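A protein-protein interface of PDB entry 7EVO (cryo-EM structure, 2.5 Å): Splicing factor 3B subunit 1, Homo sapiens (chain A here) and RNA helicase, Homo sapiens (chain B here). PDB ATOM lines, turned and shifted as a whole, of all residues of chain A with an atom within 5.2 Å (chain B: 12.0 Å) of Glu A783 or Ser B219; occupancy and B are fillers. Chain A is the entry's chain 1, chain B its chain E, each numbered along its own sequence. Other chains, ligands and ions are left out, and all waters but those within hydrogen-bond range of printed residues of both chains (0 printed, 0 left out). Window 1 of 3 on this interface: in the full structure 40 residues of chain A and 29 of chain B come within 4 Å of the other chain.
O of Asp B222 lies within hydrogen-bond range of NZ of Lys A741 (2.7 Å).
The side-chain amino group (NZ) of Lys A741 is in hydrogen-bond range of the backbone carbonyl oxygen (O) of Asp B224, at 3.2 Å.
OD2 of Asp B226 lies within salt-bridge range of NZ of Lys B216 (3.998 Å).
OE2 of Glu A783 lies within salt-bridge range of NH2 of Arg A828.
Among the printed residues, pairs that only touch across the chains: Glu A783 with Trp B218 (3.2 Å), Lys A741 with Ser B219 (3.2 Å), Asp A781 with Lys B216 (3.6 Å), Ile A787 with Leu B220 (3.8 Å), Met A784 with Trp B218 (3.8 Å), Glu A783 with Ser B219 (3.9 Å), Glu A783 with Leu B220 (3.96 Å) and Lys A741 with Asp B223 (3.98 Å).
Glu A783 touches three residues of chain B.
Of chain A, only Lys A741 and Glu A783 come within 4 Å of Ser B219.
Of the printed residues of chain B, Asp A781 touches Lys B216.
Glu A782 touches none of the printed residues of chain B.
Of chain B, only Trp B218 (3.8 Å) comes within 4 Å of Met A784.
Of the printed residues of chain B, Ile A787 touches Leu B220.
Of the printed residues of chain A, Trp B218 touches Glu A783 (3.2 Å) and Met A784 (3.8 Å).
Of the printed residues of chain A, Asp B222 touches Lys A741.
Printed residues of chain B within 4 Å of Lys A741: Ser B219 (3.2 Å), Asp B222 (2.7 Å), Asp B223 (3.98 Å) and Asp B224 (3.2 Å).
Val A788 touches none of the printed residues of chain B.
Arg A828 touches none of the printed residues of chain B.
The nearest printed residue of chain A that does not touch Ser B219 is Arg A828 (5.6 Å).
Of the 10 printed residues of chain A, 5 touch a printed residue of chain B.
Printed residues of chain A that touch a printed residue of chain B: Lys A741, Asp A781, Glu A783, Met A784 and Ile A787.
Hydrophobic or aromatic side chains of chain A that line the printed part of chain B: Ile A787.
Of the 13 printed residues of chain B, 7 touch a printed residue of chain A.
Printed residues of chain B that touch a printed residue of chain A: Lys B216, Trp B218, Ser B219, Leu B220, Asp B222, Asp B223 and Asp B224.
Hydrophobic or aromatic side chains of chain B that line the printed part of chain A: Trp B218 and Leu B220.
Among the printed residues, 10 pairs touch across the chains.
Among the printed residues, no Asp or Glu carboxylate lies within 4 Å of a Lys or Arg side-chain nitrogen of the other chain.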
ATOM      1  N   LYS A 741      26.698   1.111 -19.306  1.00  0.00           N
ATOM      2  CA  LYS A 741      27.580   0.677 -18.191  1.00  0.00           C
ATOM      3  C   LYS A 741      27.760   1.849 -17.218  1.00  0.00           C
ATOM      4  O   LYS A 741      27.589   1.631 -16.007  1.00  0.00           O
ATOM      5  CB  LYS A 741      28.924   0.180 -18.729  1.00  0.00           C
ATOM      6  CG  LYS A 741      29.696  -0.725 -17.780  1.00  0.00           C
ATOM      7  CD  LYS A 741      31.077  -1.085 -18.271  1.00  0.00           C
ATOM      8  CE  LYS A 741      31.846  -1.933 -17.282  1.00  0.00           C
ATOM      9  NZ  LYS A 741      33.281  -2.022 -17.637  1.00  0.00           N
ATOM     10  N   ASP A 781      19.575  -6.086 -20.651  1.00  0.00           N
ATOM     11  CA  ASP A 781      20.750  -6.553 -19.928  1.00  0.00           C
ATOM     12  C   ASP A 781      20.359  -7.045 -18.540  1.00  0.00           C
ATOM     13  O   ASP A 781      19.391  -6.564 -17.946  1.00  0.00           O
ATOM     14  CB  ASP A 781      21.780  -5.429 -19.825  1.00  0.00           C
ATOM     15  CG  ASP A 781      21.820  -4.565 -21.070  1.00  0.00           C
ATOM     16  OD1 ASP A 781      21.958  -5.124 -22.177  1.00  0.00           O
ATOM     17  OD2 ASP A 781      21.711  -3.327 -20.942  1.00  0.00           O
ATOM     18  N   GLU A 782      21.118  -8.013 -18.023  1.00  0.00           N
ATOM     19  CA  GLU A 782      20.737  -8.639 -16.762  1.00  0.00           C
ATOM     20  C   GLU A 782      21.511  -8.049 -15.589  1.00  0.00           C
ATOM     21  O   GLU A 782      20.978  -7.955 -14.477  1.00  0.00           O
ATOM     22  CB  GLU A 782      20.923 -10.151 -16.851  1.00  0.00           C
ATOM     23  CG  GLU A 782      19.628 -10.899 -17.129  1.00  0.00           C
ATOM     24  CD  GLU A 782      19.134 -10.698 -18.550  1.00  0.00           C
ATOM     25  OE1 GLU A 782      19.938 -10.866 -19.491  1.00  0.00           O
ATOM     26  OE2 GLU A 782      17.942 -10.369 -18.724  1.00  0.00           O
ATOM     27  N   GLU A 783      22.735  -7.601 -15.878  1.00  0.00           N
ATOM     28  CA  GLU A 783      23.551  -6.883 -14.870  1.00  0.00           C
ATOM     29  C   GLU A 783      22.739  -5.642 -14.489  1.00  0.00           C
ATOM     30  O   GLU A 783      22.595  -5.368 -13.282  1.00  0.00           O
ATOM     31  CB  GLU A 783      24.891  -6.475 -15.484  1.00  0.00           C
ATOM     32  CG  GLU A 783      25.939  -7.570 -15.431  1.00  0.00           C
ATOM     33  CD  GLU A 783      26.767  -7.580 -14.159  1.00  0.00           C
ATOM     34  OE1 GLU A 783      27.030  -6.487 -13.622  1.00  0.00           O
ATOM     35  OE2 GLU A 783      27.143  -8.680 -13.705  1.00  0.00           O
ATOM     36  N   MET A 784      22.191  -4.961 -15.503  1.00  0.00           N
ATOM     37  CA  MET A 784      21.361  -3.781 -15.294  1.00  0.00           C
ATOM     38  C   MET A 784      20.153  -4.110 -14.428  1.00  0.00           C
ATOM     39  O   MET A 784      19.771  -3.321 -13.557  1.00  0.00           O
ATOM     40  CB  MET A 784      20.919  -3.210 -16.640  1.00  0.00           C
ATOM     41  CG  MET A 784      20.180  -1.889 -16.541  1.00  0.00           C
ATOM     42  SD  MET A 784      21.289  -0.498 -16.263  1.00  0.00           S
ATOM     43  CE  MET A 784      20.949  -0.149 -14.542  1.00  0.00           C
ATOM     44  N   LYS A 785      19.544  -5.280 -14.647  1.00  0.00           N
ATOM     45  CA  LYS A 785      18.406  -5.687 -13.828  1.00  0.00           C
ATOM     46  C   LYS A 785      18.817  -5.894 -12.377  1.00  0.00           C
ATOM     47  O   LYS A 785      18.097  -5.491 -11.456  1.00  0.00           O
ATOM     48  CB  LYS A 785      17.781  -6.963 -14.393  1.00  0.00           C
ATOM     49  CG  LYS A 785      17.068  -6.776 -15.722  1.00  0.00           C
ATOM     50  CD  LYS A 785      15.795  -7.602 -15.783  1.00  0.00           C
ATOM     51  CE  LYS A 785      15.671  -8.346 -17.100  1.00  0.00           C
ATOM     52  NZ  LYS A 785      14.666  -9.442 -17.014  1.00  0.00           N
ATOM     53  N   LYS A 786      19.971  -6.524 -12.152  1.00  0.00           N
ATOM     54  CA  LYS A 786      20.454  -6.733 -10.790  1.00  0.00           C
ATOM     55  C   LYS A 786      20.727  -5.407 -10.087  1.00  0.00           C
ATOM     56  O   LYS A 786      20.347  -5.219  -8.923  1.00  0.00           O
ATOM     57  CB  LYS A 786      21.707  -7.607 -10.816  1.00  0.00           C
ATOM     58  CG  LYS A 786      22.685  -7.364  -9.682  1.00  0.00           C
ATOM     59  CD  LYS A 786      23.828  -8.363  -9.740  1.00  0.00           C
ATOM     60  CE  LYS A 786      25.040  -7.874  -8.968  1.00  0.00           C
ATOM     61  NZ  LYS A 786      26.154  -8.856  -9.030  1.00  0.00           N
ATOM     62  N   ILE A 787      21.373  -4.469 -10.784  1.00  0.00           N
ATOM     63  CA  ILE A 787      21.641  -3.159 -10.198  1.00  0.00           C
ATOM     64  C   ILE A 787      20.339  -2.423  -9.900  1.00  0.00           C
ATOM     65  O   ILE A 787      20.194  -1.805  -8.839  1.00  0.00           O
ATOM     66  CB  ILE A 787      22.559  -2.337 -11.122  1.00  0.00           C
ATOM     67  CG1 ILE A 787      23.914  -3.028 -11.289  1.00  0.00           C
ATOM     68  CG2 ILE A 787      22.735  -0.926 -10.584  1.00  0.00           C
ATOM     69  CD1 ILE A 787      24.838  -2.864 -10.109  1.00  0.00           C
ATOM     70  N   VAL A 788      19.377  -2.475 -10.824  1.00  0.00           N
ATOM     71  CA  VAL A 788      18.098  -1.802 -10.618  1.00  0.00           C
ATOM     72  C   VAL A 788      17.368  -2.391  -9.419  1.00  0.00           C
ATOM     73  O   VAL A 788      16.784  -1.661  -8.608  1.00  0.00           O
ATOM     74  CB  VAL A 788      17.249  -1.881 -11.900  1.00  0.00           C
ATOM     75  CG1 VAL A 788      15.779  -1.735 -11.579  1.00  0.00           C
ATOM     76  CG2 VAL A 788      17.683  -0.815 -12.887  1.00  0.00           C
ATOM     77  N   ARG A 828      20.229 -16.152 -11.802  1.00  0.00           N
ATOM     78  CA  ARG A 828      21.112 -15.125 -11.258  1.00  0.00           C
ATOM     79  C   ARG A 828      20.340 -14.119 -10.411  1.00  0.00           C
ATOM     80  O   ARG A 828      20.715 -13.836  -9.267  1.00  0.00           O
ATOM     81  CB  ARG A 828      21.855 -14.422 -12.394  1.00  0.00           C
ATOM     82  CG  ARG A 828      23.056 -13.610 -11.937  1.00  0.00           C
ATOM     83  CD  ARG A 828      23.802 -13.011 -13.116  1.00  0.00           C
ATOM     84  NE  ARG A 828      24.761 -11.997 -12.688  1.00  0.00           N
ATOM     85  CZ  ARG A 828      26.035 -12.249 -12.405  1.00  0.00           C
ATOM     86  NH1 ARG A 828      26.505 -13.484 -12.502  1.00  0.00           N
ATOM     87  NH2 ARG A 828      26.838 -11.266 -12.021  1.00  0.00           N
ATOM     88  N   GLY B 215      20.895  -8.057 -26.024  1.00  0.00           N
ATOM     89  CA  GLY B 215      21.366  -8.435 -24.679  1.00  0.00           C
ATOM     90  C   GLY B 215      22.879  -8.489 -24.599  1.00  0.00           C
ATOM     91  O   GLY B 215      23.415  -9.602 -24.367  1.00  0.00           O
ATOM     92  N   LYS B 216      23.548  -7.347 -24.777  1.00  0.00           N
ATOM     93  CA  LYS B 216      25.039  -7.282 -24.716  1.00  0.00           C
ATOM     94  C   LYS B 216      25.504  -7.635 -23.297  1.00  0.00           C
ATOM     95  O   LYS B 216      24.831  -7.225 -22.345  1.00  0.00           O
ATOM     96  CB  LYS B 216      25.540  -5.900 -25.144  1.00  0.00           C
ATOM     97  CG  LYS B 216      25.296  -5.550 -26.609  1.00  0.00           C
ATOM     98  CD  LYS B 216      25.793  -4.175 -26.995  1.00  0.00           C
ATOM     99  CE  LYS B 216      25.408  -3.794 -28.411  1.00  0.00           C
ATOM    100  NZ  LYS B 216      25.924  -2.453 -28.779  1.00  0.00           N
ATOM    101  N   LYS B 217      26.616  -8.367 -23.179  1.00  0.00           N
ATOM    102  CA  LYS B 217      27.121  -8.799 -21.847  1.00  0.00           C
ATOM    103  C   LYS B 217      28.334  -7.961 -21.421  1.00  0.00           C
ATOM    104  O   LYS B 217      29.351  -7.971 -22.139  1.00  0.00           O
ATOM    105  CB  LYS B 217      27.446 -10.295 -21.856  1.00  0.00           C
ATOM    106  CG  LYS B 217      26.250 -11.209 -22.080  1.00  0.00           C
ATOM    107  CD  LYS B 217      26.603 -12.681 -22.085  1.00  0.00           C
ATOM    108  CE  LYS B 217      25.429 -13.564 -22.450  1.00  0.00           C
ATOM    109  NZ  LYS B 217      24.847 -13.187 -23.760  1.00  0.00           N
ATOM    110  N   TRP B 218      28.204  -7.275 -20.283  1.00  0.00           N
ATOM    111  CA  TRP B 218      29.285  -6.444 -19.684  1.00  0.00           C
ATOM    112  C   TRP B 218      29.273  -6.656 -18.171  1.00  0.00           C
ATOM    113  O   TRP B 218      28.219  -7.063 -17.645  1.00  0.00           O
ATOM    114  CB  TRP B 218      29.142  -4.965 -20.076  1.00  0.00           C
ATOM    115  CG  TRP B 218      27.751  -4.420 -19.970  1.00  0.00           C
ATOM    116  CD1 TRP B 218      26.879  -4.194 -20.995  1.00  0.00           C
ATOM    117  CD2 TRP B 218      27.067  -4.026 -18.770  1.00  0.00           C
ATOM    118  NE1 TRP B 218      25.703  -3.681 -20.516  1.00  0.00           N
ATOM    119  CE2 TRP B 218      25.787  -3.568 -19.156  1.00  0.00           C
ATOM    120  CE3 TRP B 218      27.409  -4.005 -17.412  1.00  0.00           C
ATOM    121  CZ2 TRP B 218      24.852  -3.105 -18.231  1.00  0.00           C
ATOM    122  CZ3 TRP B 218      26.486  -3.544 -16.500  1.00  0.00           C
ATOM    123  CH2 TRP B 218      25.225  -3.101 -16.905  1.00  0.00           C
ATOM    124  N   SER B 219      30.399  -6.437 -17.496  1.00  0.00           N
ATOM    125  CA  SER B 219      30.491  -6.630 -16.025  1.00  0.00           C
ATOM    126  C   SER B 219      31.138  -5.408 -15.376  1.00  0.00           C
ATOM    127  O   SER B 219      32.094  -4.875 -15.954  1.00  0.00           O
ATOM    128  CB  SER B 219      31.236  -7.892 -15.705  1.00  0.00           C
ATOM    129  OG  SER B 219      31.003  -8.283 -14.356  1.00  0.00           O
ATOM    130  N   LEU B 220      30.664  -5.016 -14.192  1.00  0.00           N
ATOM    131  CA  LEU B 220      31.239  -3.882 -13.426  1.00  0.00           C
ATOM    132  C   LEU B 220      32.567  -4.317 -12.810  1.00  0.00           C
ATOM    133  O   LEU B 220      33.217  -3.475 -12.154  1.00  0.00           O
ATOM    134  CB  LEU B 220      30.241  -3.412 -12.366  1.00  0.00           C
ATOM    135  CG  LEU B 220      29.073  -2.573 -12.885  1.00  0.00           C
ATOM    136  CD1 LEU B 220      28.180  -2.127 -11.739  1.00  0.00           C
ATOM    137  CD2 LEU B 220      29.552  -1.359 -13.670  1.00  0.00           C
ATOM    138  N   GLU B 221      32.967  -5.570 -13.041  1.00  0.00           N
ATOM    139  CA  GLU B 221      34.235  -6.106 -12.479  1.00  0.00           C
ATOM    140  C   GLU B 221      35.364  -5.968 -13.509  1.00  0.00           C
ATOM    141  O   GLU B 221      36.470  -6.458 -13.224  1.00  0.00           O
ATOM    142  CB  GLU B 221      34.052  -7.569 -12.080  1.00  0.00           C
ATOM    143  CG  GLU B 221      32.850  -7.801 -11.182  1.00  0.00           C
ATOM    144  CD  GLU B 221      32.405  -9.250 -11.091  1.00  0.00           C
ATOM    145  OE1 GLU B 221      33.121 -10.120 -11.626  1.00  0.00           O
ATOM    146  OE2 GLU B 221      31.340  -9.503 -10.493  1.00  0.00           O
ATOM    147  N   ASP B 222      35.098  -5.304 -14.639  1.00  0.00           N
ATOM    148  CA  ASP B 222      36.120  -5.125 -15.706  1.00  0.00           C
ATOM    149  C   ASP B 222      36.159  -3.661 -16.155  1.00  0.00           C
ATOM    150  O   ASP B 222      35.159  -2.953 -15.944  1.00  0.00           O
ATOM    151  CB  ASP B 222      35.832  -6.019 -16.915  1.00  0.00           C
ATOM    152  CG  ASP B 222      35.662  -7.489 -16.573  1.00  0.00           C
ATOM    153  OD1 ASP B 222      36.506  -8.019 -15.829  1.00  0.00           O
ATOM    154  OD2 ASP B 222      34.686  -8.091 -17.061  1.00  0.00           O
ATOM    155  N   ASP B 223      37.296  -3.225 -16.709  1.00  0.00           N
ATOM    156  CA  ASP B 223      37.461  -1.838 -17.222  1.00  0.00           C
ATOM    157  C   ASP B 223      37.105  -1.810 -18.713  1.00  0.00           C
ATOM    158  O   ASP B 223      37.179  -0.725 -19.319  1.00  0.00           O
ATOM    159  CB  ASP B 223      38.896  -1.337 -17.045  1.00  0.00           C
ATOM    160  CG  ASP B 223      39.605  -1.912 -15.834  1.00  0.00           C
ATOM    161  OD1 ASP B 223      38.918  -2.494 -14.973  1.00  0.00           O
ATOM    162  OD2 ASP B 223      40.841  -1.778 -15.764  1.00  0.00           O
ATOM    163  N   ASP B 224      36.749  -2.970 -19.273  1.00  0.00           N
ATOM    164  CA  ASP B 224      36.418  -3.107 -20.716  1.00  0.00           C
ATOM    165  C   ASP B 224      35.269  -2.170 -21.106  1.00  0.00           C
ATOM    166  O   ASP B 224      34.126  -2.422 -20.683  1.00  0.00           O
ATOM    167  CB  ASP B 224      36.073  -4.555 -21.072  1.00  0.00           C
ATOM    168  CG  ASP B 224      37.038  -5.570 -20.486  1.00  0.00           C
ATOM    169  OD1 ASP B 224      38.078  -5.146 -19.947  1.00  0.00           O
ATOM    170  OD2 ASP B 224      36.738  -6.778 -20.570  1.00  0.00           O
ATOM    171  N   ASP B 225      35.584  -1.122 -21.873  1.00  0.00           N
ATOM    172  CA  ASP B 225      34.574  -0.182 -22.409  1.00  0.00           C
ATOM    173  C   ASP B 225      33.952  -0.857 -23.630  1.00  0.00           C
ATOM    174  O   ASP B 225      34.715  -1.509 -24.374  1.00  0.00           O
ATOM    175  CB  ASP B 225      35.202   1.160 -22.776  1.00  0.00           C
ATOM    176  CG  ASP B 225      34.177   2.251 -23.024  1.00  0.00           C
ATOM    177  OD1 ASP B 225      34.444   3.120 -23.881  1.00  0.00           O
ATOM    178  OD2 ASP B 225      33.124   2.229 -22.352  1.00  0.00           O
ATOM    179  N   ASP B 226      32.651  -0.690 -23.865  1.00  0.00           N
ATOM    180  CA  ASP B 226      32.009  -1.363 -25.024  1.00  0.00           C
ATOM    181  C   ASP B 226      32.304  -0.555 -26.289  1.00  0.00           C
ATOM    182  O   ASP B 226      31.792   0.578 -26.401  1.00  0.00           O
ATOM    183  CB  ASP B 226      30.513  -1.568 -24.809  1.00  0.00           C
ATOM    184  CG  ASP B 226      29.892  -2.510 -25.830  1.00  0.00           C
ATOM    185  OD1 ASP B 226      30.657  -3.149 -26.590  1.00  0.00           O
ATOM    186  OD2 ASP B 226      28.643  -2.609 -25.852  1.00  0.00           O
ATOM    187  N   GLU B 227      33.093  -1.125 -27.204  1.00  0.00           N
ATOM    188  CA  GLU B 227      33.464  -0.460 -28.477  1.00  0.00           C
ATOM    189  C   GLU B 227      34.021   0.931 -28.168  1.00  0.00           C
ATOM    190  O   GLU B 227      34.958   1.000 -27.352  1.00  0.00           O
ATOM    191  CB  GLU B 227      32.244  -0.484 -29.407  1.00  0.00           C
ATOM    192  CG  GLU B 227      32.593  -0.743 -30.868  1.00  0.00           C
ATOM    193  CD  GLU B 227      33.309  -2.068 -31.085  1.00  0.00           C
ATOM    194  OE1 GLU B 227      33.923  -2.570 -30.117  1.00  0.00           O
ATOM    195  OE2 GLU B 227      33.256  -2.600 -32.227  1.00  0.00           O
